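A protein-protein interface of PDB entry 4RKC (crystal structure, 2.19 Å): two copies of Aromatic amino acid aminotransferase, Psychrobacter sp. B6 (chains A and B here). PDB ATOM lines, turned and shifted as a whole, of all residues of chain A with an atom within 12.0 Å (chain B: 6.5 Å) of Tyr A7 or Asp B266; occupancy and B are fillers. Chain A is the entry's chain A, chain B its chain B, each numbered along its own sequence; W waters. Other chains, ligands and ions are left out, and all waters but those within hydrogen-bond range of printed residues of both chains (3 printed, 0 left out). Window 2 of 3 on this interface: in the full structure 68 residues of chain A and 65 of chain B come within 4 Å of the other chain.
Hydrophobic or aromatic side chains of chain B that line the printed part of chain A: Pro B263 and Val B271.
Along chain B the printed residues that touch a printed residue of chain A span positions 262 to 274.
Hydrophobic or aromatic side chains of chain A that line the printed part of chain B: Met A1, Phe A2, Ile A5, Tyr A7 and Tyr A8.
No position is printed for both chains.
Of the 18 pairs that touch across the chains among the printed residues, none has its exchanged pair printed and touching as well.
Met A1 touches Pro B263 (CB to CG, 3.8 Å).
Phe A2 touches Cys B262.
O of Phe A2 touches CD of Arg B270, at 3.7 Å.
CG2 of Val B271 touches CG of Phe A2 (3.5 Å).
Glu A3 touches Glu B267 (OE1 to OE2, 3.6 Å).
CG2 of Ile A5 touches CG of Gln B274 (3.3 Å).
O of Asp A6 touches O of Arg B270, at 3.8 Å.
Tyr A7 touches Arg B270.
Gly B273 touches Tyr A8.
Tyr A8 touches Gln B274.
Asp B266 touches just one residue of chain A: Tyr A7 (2.5 Å).
No residue of chain A comes within 4 Å of Thr B264.
No residue of chain A comes within 4 Å of Val B265.
Glu B267 touches just these residues of chain A: Met A1, Phe A2 and Glu A3.
Printed residues of chain A within 4 Å of Glu B269: Tyr A7.
Gly B273 touches just one residue of chain A: Tyr A8.
Of the printed residues of chain A, Val B271 touches Phe A2.
Printed residues of chain B within 4 Å of Asp A6: Arg B270 (3.8 Å) and Gln B274 (2.9 Å).
Of the printed residues of chain B, Met A1 touches Pro B263 and Glu B267.
Leu B94 touches none of the printed residues of chain A.
Asp A11 touches none of the printed residues of chain B.
OE2 of Glu B267 lies within hydrogen-bond range of N of Met A1 (2.7 Å).
The backbone NH (N) of Phe A2 is in hydrogen-bond range of the side-chain carboxylate (OE2) of Glu B267.
The backbone carbonyl oxygen (O) of Glu A3 lies close to the guanidinium group (NH1) of Arg B270 (3.4 Å).
O of Ile A5 is in hydrogen-bond range of NH1 of Arg B270, at 2.8 Å.
NE2 of Gln B274 is in hydrogen-bond range of O of Asp A6 (2.9 Å).
The side-chain carboxylate of Asp B266 lies within hydrogen-bond range of the side-chain hydroxyl of Tyr A7 (2.5 Å).
The backbone carbonyl oxygen (O) of Tyr A7 is in hydrogen-bond range of the side-chain amide nitrogen (NE2) of Gln B274 (3.2 Å).
The side-chain carboxylate (OE1) of Glu A3 lies within hydrogen-bond range of the backbone NH (N) of Met A1 (2.9 Å).
O of Leu B94 sits at hydrogen-bond distance from N of Cys B262, 2.7 Å away.
The side-chain carboxylate (OE1) of Glu B267 lies within hydrogen-bond range of the side-chain hydroxyl (OG1) of Thr B264 (2.7 Å).
The guanidinium group (NE) of Arg B270 is in salt-bridge range of the side-chain carboxylate (OD2) of Asp B266 (3.0 Å).
Water W1 lies within hydrogen-bond range of the side-chain carboxylate of Glu B267 (2.7 Å), the side-chain carboxylate of Glu A3 (3.2 Å) and the backbone NH of Met A1 (3.5 Å).
Water W3 lies within hydrogen-bond range of NE2 of Gln B274 and O of Tyr A7.
Water W2 bridges O of Glu B269 (2.8 Å) and N of Tyr A8 (2.9 Å).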
ATOM      1  N   MET A   1      -4.821  -4.971 -22.163  1.00  0.00           N
ATOM      2  CA  MET A   1      -6.101  -4.228 -22.261  1.00  0.00           C
ATOM      3  C   MET A   1      -6.412  -3.365 -21.030  1.00  0.00           C
ATOM      4  O   MET A   1      -6.966  -2.274 -21.151  1.00  0.00           O
ATOM      5  CB  MET A   1      -7.210  -5.226 -22.379  1.00  0.00           C
ATOM      6  CG  MET A   1      -8.597  -4.620 -22.330  1.00  0.00           C
ATOM      7  SD  MET A   1      -8.944  -3.794 -23.907  1.00  0.00           S
ATOM      8  CE  MET A   1     -10.382  -2.829 -23.399  1.00  0.00           C
ATOM      9  N   PHE A   2      -6.081  -3.842 -19.844  1.00  0.00           N
ATOM     10  CA  PHE A   2      -6.480  -3.175 -18.616  1.00  0.00           C
ATOM     11  C   PHE A   2      -5.291  -2.745 -17.761  1.00  0.00           C
ATOM     12  O   PHE A   2      -5.419  -2.577 -16.536  1.00  0.00           O
ATOM     13  CB  PHE A   2      -7.379  -4.151 -17.843  1.00  0.00           C
ATOM     14  CG  PHE A   2      -8.665  -4.502 -18.558  1.00  0.00           C
ATOM     15  CD1 PHE A   2      -8.904  -5.766 -18.958  1.00  0.00           C
ATOM     16  CD2 PHE A   2      -9.624  -3.525 -18.826  1.00  0.00           C
ATOM     17  CE1 PHE A   2     -10.119  -6.099 -19.591  1.00  0.00           C
ATOM     18  CE2 PHE A   2     -10.824  -3.846 -19.453  1.00  0.00           C
ATOM     19  CZ  PHE A   2     -11.083  -5.167 -19.806  1.00  0.00           C
ATOM     20  N   GLU A   3      -4.142  -2.532 -18.399  1.00  0.00           N
ATOM     21  CA  GLU A   3      -2.922  -2.276 -17.658  1.00  0.00           C
ATOM     22  C   GLU A   3      -2.984  -1.009 -16.865  1.00  0.00           C
ATOM     23  O   GLU A   3      -2.308  -0.902 -15.851  1.00  0.00           O
ATOM     24  CB  GLU A   3      -1.709  -2.203 -18.555  1.00  0.00           C
ATOM     25  CG  GLU A   3      -1.377  -3.536 -19.204  1.00  0.00           C
ATOM     26  CD  GLU A   3      -2.073  -3.729 -20.547  1.00  0.00           C
ATOM     27  OE1 GLU A   3      -3.106  -3.055 -20.832  1.00  0.00           O
ATOM     28  OE2 GLU A   3      -1.611  -4.592 -21.331  1.00  0.00           O
ATOM     29  N   ARG A   4      -3.797  -0.052 -17.289  1.00  0.00           N
ATOM     30  CA  ARG A   4      -3.840   1.222 -16.580  1.00  0.00           C
ATOM     31  C   ARG A   4      -4.839   1.212 -15.444  1.00  0.00           C
ATOM     32  O   ARG A   4      -4.987   2.210 -14.751  1.00  0.00           O
ATOM     33  CB  ARG A   4      -4.368   2.268 -17.520  1.00  0.00           C
ATOM     34  CG  ARG A   4      -3.458   2.629 -18.632  1.00  0.00           C
ATOM     35  CD  ARG A   4      -4.049   3.874 -19.271  1.00  0.00           C
ATOM     36  NE  ARG A   4      -3.259   4.339 -20.427  1.00  0.00           N
ATOM     37  CZ  ARG A   4      -3.318   3.799 -21.644  1.00  0.00           C
ATOM     38  NH1 ARG A   4      -4.106   2.741 -21.892  1.00  0.00           N
ATOM     39  NH2 ARG A   4      -2.610   4.340 -22.625  1.00  0.00           N
ATOM     40  N   ILE A   5      -5.634   0.153 -15.332  1.00  0.00           N
ATOM     41  CA  ILE A   5      -6.689   0.131 -14.341  1.00  0.00           C
ATOM     42  C   ILE A   5      -5.875  -0.002 -13.057  1.00  0.00           C
ATOM     43  O   ILE A   5      -5.165  -0.948 -12.934  1.00  0.00           O
ATOM     44  CB  ILE A   5      -7.623  -1.105 -14.506  1.00  0.00           C
ATOM     45  CG1 ILE A   5      -8.342  -1.208 -15.848  1.00  0.00           C
ATOM     46  CG2 ILE A   5      -8.439  -1.362 -13.264  1.00  0.00           C
ATOM     47  CD1 ILE A   5      -8.924   0.033 -16.450  1.00  0.00           C
ATOM     48  N   ASP A   6      -5.987   0.944 -12.122  1.00  0.00           N
ATOM     49  CA  ASP A   6      -5.316   0.871 -10.813  1.00  0.00           C
ATOM     50  C   ASP A   6      -5.730  -0.347 -10.060  1.00  0.00           C
ATOM     51  O   ASP A   6      -6.888  -0.795 -10.132  1.00  0.00           O
ATOM     52  CB  ASP A   6      -5.762   2.010  -9.873  1.00  0.00           C
ATOM     53  CG  ASP A   6      -5.516   3.470 -10.434  1.00  0.00           C
ATOM     54  OD1 ASP A   6      -5.955   4.442  -9.756  1.00  0.00           O
ATOM     55  OD2 ASP A   6      -4.917   3.692 -11.482  1.00  0.00           O
ATOM     56  N   TYR A   7      -4.790  -0.875  -9.281  1.00  0.00           N
ATOM     57  CA  TYR A   7      -5.151  -1.836  -8.251  1.00  0.00           C
ATOM     58  C   TYR A   7      -6.161  -1.148  -7.349  1.00  0.00           C
ATOM     59  O   TYR A   7      -6.162   0.071  -7.237  1.00  0.00           O
ATOM     60  CB  TYR A   7      -3.949  -2.195  -7.421  1.00  0.00           C
ATOM     61  CG  TYR A   7      -2.882  -2.871  -8.229  1.00  0.00           C
ATOM     62  CD1 TYR A   7      -3.110  -4.134  -8.780  1.00  0.00           C
ATOM     63  CD2 TYR A   7      -1.649  -2.250  -8.477  1.00  0.00           C
ATOM     64  CE1 TYR A   7      -2.144  -4.786  -9.540  1.00  0.00           C
ATOM     65  CE2 TYR A   7      -0.653  -2.903  -9.250  1.00  0.00           C
ATOM     66  CZ  TYR A   7      -0.910  -4.184  -9.752  1.00  0.00           C
ATOM     67  OH  TYR A   7       0.008  -4.868 -10.501  1.00  0.00           O
ATOM     68  N   TYR A   8      -7.016  -1.939  -6.707  1.00  0.00           N
ATOM     69  CA  TYR A   8      -7.845  -1.413  -5.650  1.00  0.00           C
ATOM     70  C   TYR A   8      -7.102  -1.720  -4.342  1.00  0.00           C
ATOM     71  O   TYR A   8      -6.752  -2.875  -4.082  1.00  0.00           O
ATOM     72  CB  TYR A   8      -9.208  -2.101  -5.693  1.00  0.00           C
ATOM     73  CG  TYR A   8     -10.143  -1.692  -4.589  1.00  0.00           C
ATOM     74  CD1 TYR A   8     -10.258  -0.338  -4.200  1.00  0.00           C
ATOM     75  CD2 TYR A   8     -10.940  -2.643  -3.948  1.00  0.00           C
ATOM     76  CE1 TYR A   8     -11.129   0.046  -3.198  1.00  0.00           C
ATOM     77  CE2 TYR A   8     -11.805  -2.269  -2.933  1.00  0.00           C
ATOM     78  CZ  TYR A   8     -11.899  -0.923  -2.575  1.00  0.00           C
ATOM     79  OH  TYR A   8     -12.778  -0.560  -1.588  1.00  0.00           O
ATOM     80  N   ALA A   9      -6.839  -0.702  -3.524  1.00  0.00           N
ATOM     81  CA  ALA A   9      -6.038  -0.909  -2.305  1.00  0.00           C
ATOM     82  C   ALA A   9      -6.760  -1.858  -1.365  1.00  0.00           C
ATOM     83  O   ALA A   9      -6.171  -2.416  -0.452  1.00  0.00           O
ATOM     84  CB  ALA A   9      -5.756   0.425  -1.601  1.00  0.00           C
ATOM     85  N   GLY A  10      -8.055  -2.010  -1.593  1.00  0.00           N
ATOM     86  CA  GLY A  10      -8.890  -2.800  -0.751  1.00  0.00           C
ATOM     87  C   GLY A  10      -9.641  -1.878   0.194  1.00  0.00           C
ATOM     88  O   GLY A  10      -9.245  -0.692   0.448  1.00  0.00           O
ATOM     89  N   ASP A  11     -10.737  -2.430   0.711  1.00  0.00           N
ATOM     90  CA  ASP A  11     -11.453  -1.774   1.778  1.00  0.00           C
ATOM     91  C   ASP A  11     -10.592  -1.862   3.040  1.00  0.00           C
ATOM     92  O   ASP A  11     -10.240  -2.989   3.473  1.00  0.00           O
ATOM     93  CB  ASP A  11     -12.840  -2.394   2.003  1.00  0.00           C
ATOM     94  CG  ASP A  11     -13.460  -1.930   3.304  1.00  0.00           C
ATOM     95  OD1 ASP A  11     -13.676  -0.705   3.472  1.00  0.00           O
ATOM     96  OD2 ASP A  11     -13.680  -2.791   4.180  1.00  0.00           O
ATOM     97  N   PRO A  12     -10.225  -0.678   3.602  1.00  0.00           N
ATOM     98  CA  PRO A  12      -9.501  -0.492   4.875  1.00  0.00           C
ATOM     99  C   PRO A  12      -9.917  -1.480   5.986  1.00  0.00           C
ATOM    100  O   PRO A  12      -9.075  -2.261   6.463  1.00  0.00           O
ATOM    101  CB  PRO A  12      -9.885   0.943   5.293  1.00  0.00           C
ATOM    102  CG  PRO A  12     -10.138   1.648   3.997  1.00  0.00           C
ATOM    103  CD  PRO A  12     -10.541   0.617   2.964  1.00  0.00           C
ATOM    104  N   GLU A  18      -8.864  -9.612   6.968  1.00  0.00           N
ATOM    105  CA  GLU A  18      -7.857 -10.361   6.232  1.00  0.00           C
ATOM    106  C   GLU A  18      -6.641 -10.584   7.153  1.00  0.00           C
ATOM    107  O   GLU A  18      -6.393 -11.722   7.584  1.00  0.00           O
ATOM    108  CB  GLU A  18      -7.485  -9.620   4.928  1.00  0.00           C
ATOM    109  CG  GLU A  18      -7.430 -10.484   3.664  1.00  0.00           C
ATOM    110  CD  GLU A  18      -7.742  -9.702   2.383  1.00  0.00           C
ATOM    111  OE1 GLU A  18      -8.943  -9.495   2.068  1.00  0.00           O
ATOM    112  OE2 GLU A  18      -6.788  -9.308   1.674  1.00  0.00           O
ATOM    113  N   GLY B  93      -6.642 -18.083 -14.532  1.00  0.00           N
ATOM    114  CA  GLY B  93      -6.933 -16.940 -13.675  1.00  0.00           C
ATOM    115  C   GLY B  93      -7.173 -15.672 -14.464  1.00  0.00           C
ATOM    116  O   GLY B  93      -6.774 -14.585 -14.047  1.00  0.00           O
ATOM    117  N   LEU B  94      -7.786 -15.817 -15.619  1.00  0.00           N
ATOM    118  CA  LEU B  94      -7.943 -14.688 -16.505  1.00  0.00           C
ATOM    119  C   LEU B  94      -9.401 -14.084 -16.547  1.00  0.00           C
ATOM    120  O   LEU B  94      -9.708 -13.280 -17.419  1.00  0.00           O
ATOM    121  CB  LEU B  94      -7.483 -15.087 -17.900  1.00  0.00           C
ATOM    122  CG  LEU B  94      -6.026 -15.450 -18.107  1.00  0.00           C
ATOM    123  CD1 LEU B  94      -5.815 -15.874 -19.579  1.00  0.00           C
ATOM    124  CD2 LEU B  94      -5.145 -14.261 -17.780  1.00  0.00           C
ATOM    125  N   CYS B 262      -9.670 -11.114 -19.019  1.00  0.00           N
ATOM    126  CA  CYS B 262      -8.506 -10.193 -18.993  1.00  0.00           C
ATOM    127  C   CYS B 262      -7.341 -10.846 -19.697  1.00  0.00           C
ATOM    128  O   CYS B 262      -7.263 -12.074 -19.715  1.00  0.00           O
ATOM    129  CB  CYS B 262      -8.127  -9.871 -17.566  1.00  0.00           C
ATOM    130  SG  CYS B 262      -9.474  -8.967 -16.745  1.00  0.00           S
ATOM    131  N   PRO B 263      -6.425 -10.063 -20.284  1.00  0.00           N
ATOM    132  CA  PRO B 263      -5.343 -10.856 -20.967  1.00  0.00           C
ATOM    133  C   PRO B 263      -4.235 -11.427 -20.043  1.00  0.00           C
ATOM    134  O   PRO B 263      -3.478 -12.320 -20.460  1.00  0.00           O
ATOM    135  CB  PRO B 263      -4.778  -9.863 -22.000  1.00  0.00           C
ATOM    136  CG  PRO B 263      -5.854  -8.816 -22.150  1.00  0.00           C
ATOM    137  CD  PRO B 263      -6.457  -8.678 -20.747  1.00  0.00           C
ATOM    138  N   THR B 264      -4.103 -10.918 -18.821  1.00  0.00           N
ATOM    139  CA  THR B 264      -3.132 -11.434 -17.898  1.00  0.00           C
ATOM    140  C   THR B 264      -3.731 -11.450 -16.505  1.00  0.00           C
ATOM    141  O   THR B 264      -4.749 -10.786 -16.201  1.00  0.00           O
ATOM    142  CB  THR B 264      -1.830 -10.600 -17.845  1.00  0.00           C
ATOM    143  OG1 THR B 264      -2.130  -9.263 -17.406  1.00  0.00           O
ATOM    144  CG2 THR B 264      -1.067 -10.560 -19.236  1.00  0.00           C
ATOM    145  N   VAL B 265      -3.055 -12.203 -15.652  1.00  0.00           N
ATOM    146  CA  VAL B 265      -3.461 -12.379 -14.283  1.00  0.00           C
ATOM    147  C   VAL B 265      -3.338 -11.020 -13.606  1.00  0.00           C
ATOM    148  O   VAL B 265      -4.111 -10.685 -12.720  1.00  0.00           O
ATOM    149  CB  VAL B 265      -2.544 -13.399 -13.583  1.00  0.00           C
ATOM    150  CG1 VAL B 265      -2.474 -13.128 -12.080  1.00  0.00           C
ATOM    151  CG2 VAL B 265      -3.010 -14.783 -13.904  1.00  0.00           C
ATOM    152  N   ASP B 266      -2.368 -10.218 -14.019  1.00  0.00           N
ATOM    153  CA  ASP B 266      -2.249  -8.953 -13.327  1.00  0.00           C
ATOM    154  C   ASP B 266      -3.456  -8.019 -13.657  1.00  0.00           C
ATOM    155  O   ASP B 266      -4.023  -7.340 -12.783  1.00  0.00           O
ATOM    156  CB  ASP B 266      -0.929  -8.329 -13.681  1.00  0.00           C
ATOM    157  CG  ASP B 266      -0.722  -6.996 -13.027  1.00  0.00           C
ATOM    158  OD1 ASP B 266      -0.502  -6.946 -11.784  1.00  0.00           O
ATOM    159  OD2 ASP B 266      -0.728  -5.996 -13.789  1.00  0.00           O
ATOM    160  N   GLU B 267      -3.841  -8.003 -14.923  1.00  0.00           N
ATOM    161  CA  GLU B 267      -5.040  -7.287 -15.367  1.00  0.00           C
ATOM    162  C   GLU B 267      -6.250  -7.822 -14.671  1.00  0.00           C
ATOM    163  O   GLU B 267      -7.042  -7.045 -14.205  1.00  0.00           O
ATOM    164  CB  GLU B 267      -5.210  -7.330 -16.882  1.00  0.00           C
ATOM    165  CG  GLU B 267      -4.128  -6.474 -17.533  1.00  0.00           C
ATOM    166  CD  GLU B 267      -4.012  -6.836 -18.993  1.00  0.00           C
ATOM    167  OE1 GLU B 267      -3.264  -7.810 -19.335  1.00  0.00           O
ATOM    168  OE2 GLU B 267      -4.710  -6.159 -19.783  1.00  0.00           O
ATOM    169  N   THR B 268      -6.342  -9.147 -14.545  1.00  0.00           N
ATOM    170  CA  THR B 268      -7.387  -9.752 -13.735  1.00  0.00           C
ATOM    171  C   THR B 268      -7.449  -9.151 -12.359  1.00  0.00           C
ATOM    172  O   THR B 268      -8.498  -8.772 -11.902  1.00  0.00           O
ATOM    173  CB  THR B 268      -7.303 -11.251 -13.717  1.00  0.00           C
ATOM    174  OG1 THR B 268      -7.134 -11.625 -15.064  1.00  0.00           O
ATOM    175  CG2 THR B 268      -8.628 -11.855 -13.231  1.00  0.00           C
ATOM    176  N   GLU B 269      -6.319  -8.988 -11.729  1.00  0.00           N
ATOM    177  CA  GLU B 269      -6.293  -8.450 -10.396  1.00  0.00           C
ATOM    178  C   GLU B 269      -6.700  -6.976 -10.352  1.00  0.00           C
ATOM    179  O   GLU B 269      -7.457  -6.546  -9.461  1.00  0.00           O
ATOM    180  CB  GLU B 269      -4.891  -8.604  -9.824  1.00  0.00           C
ATOM    181  CG  GLU B 269      -4.846  -7.977  -8.450  1.00  0.00           C
ATOM    182  CD  GLU B 269      -3.516  -8.127  -7.739  1.00  0.00           C
ATOM    183  OE1 GLU B 269      -2.634  -8.864  -8.215  1.00  0.00           O
ATOM    184  OE2 GLU B 269      -3.352  -7.483  -6.699  1.00  0.00           O
ATOM    185  N   ARG B 270      -6.192  -6.174 -11.288  1.00  0.00           N
ATOM    186  CA  ARG B 270      -6.623  -4.769 -11.294  1.00  0.00           C
ATOM    187  C   ARG B 270      -8.163  -4.688 -11.544  1.00  0.00           C
ATOM    188  O   ARG B 270      -8.834  -3.931 -10.863  1.00  0.00           O
ATOM    189  CB  ARG B 270      -5.881  -3.917 -12.328  1.00  0.00           C
ATOM    190  CG  ARG B 270      -4.355  -3.853 -12.140  1.00  0.00           C
ATOM    191  CD  ARG B 270      -3.672  -3.585 -13.482  1.00  0.00           C
ATOM    192  NE  ARG B 270      -2.214  -3.379 -13.342  1.00  0.00           N
ATOM    193  CZ  ARG B 270      -1.682  -2.263 -12.868  1.00  0.00           C
ATOM    194  NH1 ARG B 270      -2.474  -1.297 -12.465  1.00  0.00           N
ATOM    195  NH2 ARG B 270      -0.363  -2.109 -12.731  1.00  0.00           N
ATOM    196  N   VAL B 271      -8.688  -5.427 -12.529  1.00  0.00           N
ATOM    197  CA  VAL B 271     -10.116  -5.359 -12.888  1.00  0.00           C
ATOM    198  C   VAL B 271     -10.992  -5.898 -11.737  1.00  0.00           C
ATOM    199  O   VAL B 271     -11.972  -5.256 -11.299  1.00  0.00           O
ATOM    200  CB  VAL B 271     -10.386  -6.104 -14.219  1.00  0.00           C
ATOM    201  CG1 VAL B 271     -11.873  -6.162 -14.460  1.00  0.00           C
ATOM    202  CG2 VAL B 271      -9.769  -5.345 -15.395  1.00  0.00           C
ATOM    203  N   GLY B 273     -10.293  -5.929  -8.599  1.00  0.00           N
ATOM    204  CA  GLY B 273     -10.126  -4.977  -7.490  1.00  0.00           C
ATOM    205  C   GLY B 273     -11.088  -3.872  -7.769  1.00  0.00           C
ATOM    206  O   GLY B 273     -11.884  -3.553  -6.951  1.00  0.00           O
ATOM    207  N   GLN B 274     -11.078  -3.361  -8.978  1.00  0.00           N
ATOM    208  CA  GLN B 274     -11.921  -2.258  -9.306  1.00  0.00           C
ATOM    209  C   GLN B 274     -13.420  -2.641  -9.365  1.00  0.00           C
ATOM    210  O   GLN B 274     -14.248  -1.781  -9.108  1.00  0.00           O
ATOM    211  CB  GLN B 274     -11.448  -1.557 -10.661  1.00  0.00           C
ATOM    212  CG  GLN B 274     -10.107  -0.790 -10.484  1.00  0.00           C
ATOM    213  CD  GLN B 274     -10.156   0.199  -9.324  1.00  0.00           C
ATOM    214  OE1 GLN B 274     -11.185   0.819  -9.118  1.00  0.00           O
ATOM    215  NE2 GLN B 274      -9.073   0.357  -8.576  1.00  0.00           N
HETATM  216  O   HOH W   1      -2.561  -7.570 -21.918  1.00  0.00           O
HETATM  217  O   HOH W   2      -6.711  -4.740  -7.462  1.00  0.00           O
HETATM  218  O   HOH W   3      -8.641   2.200  -6.566  1.00  0.00           O
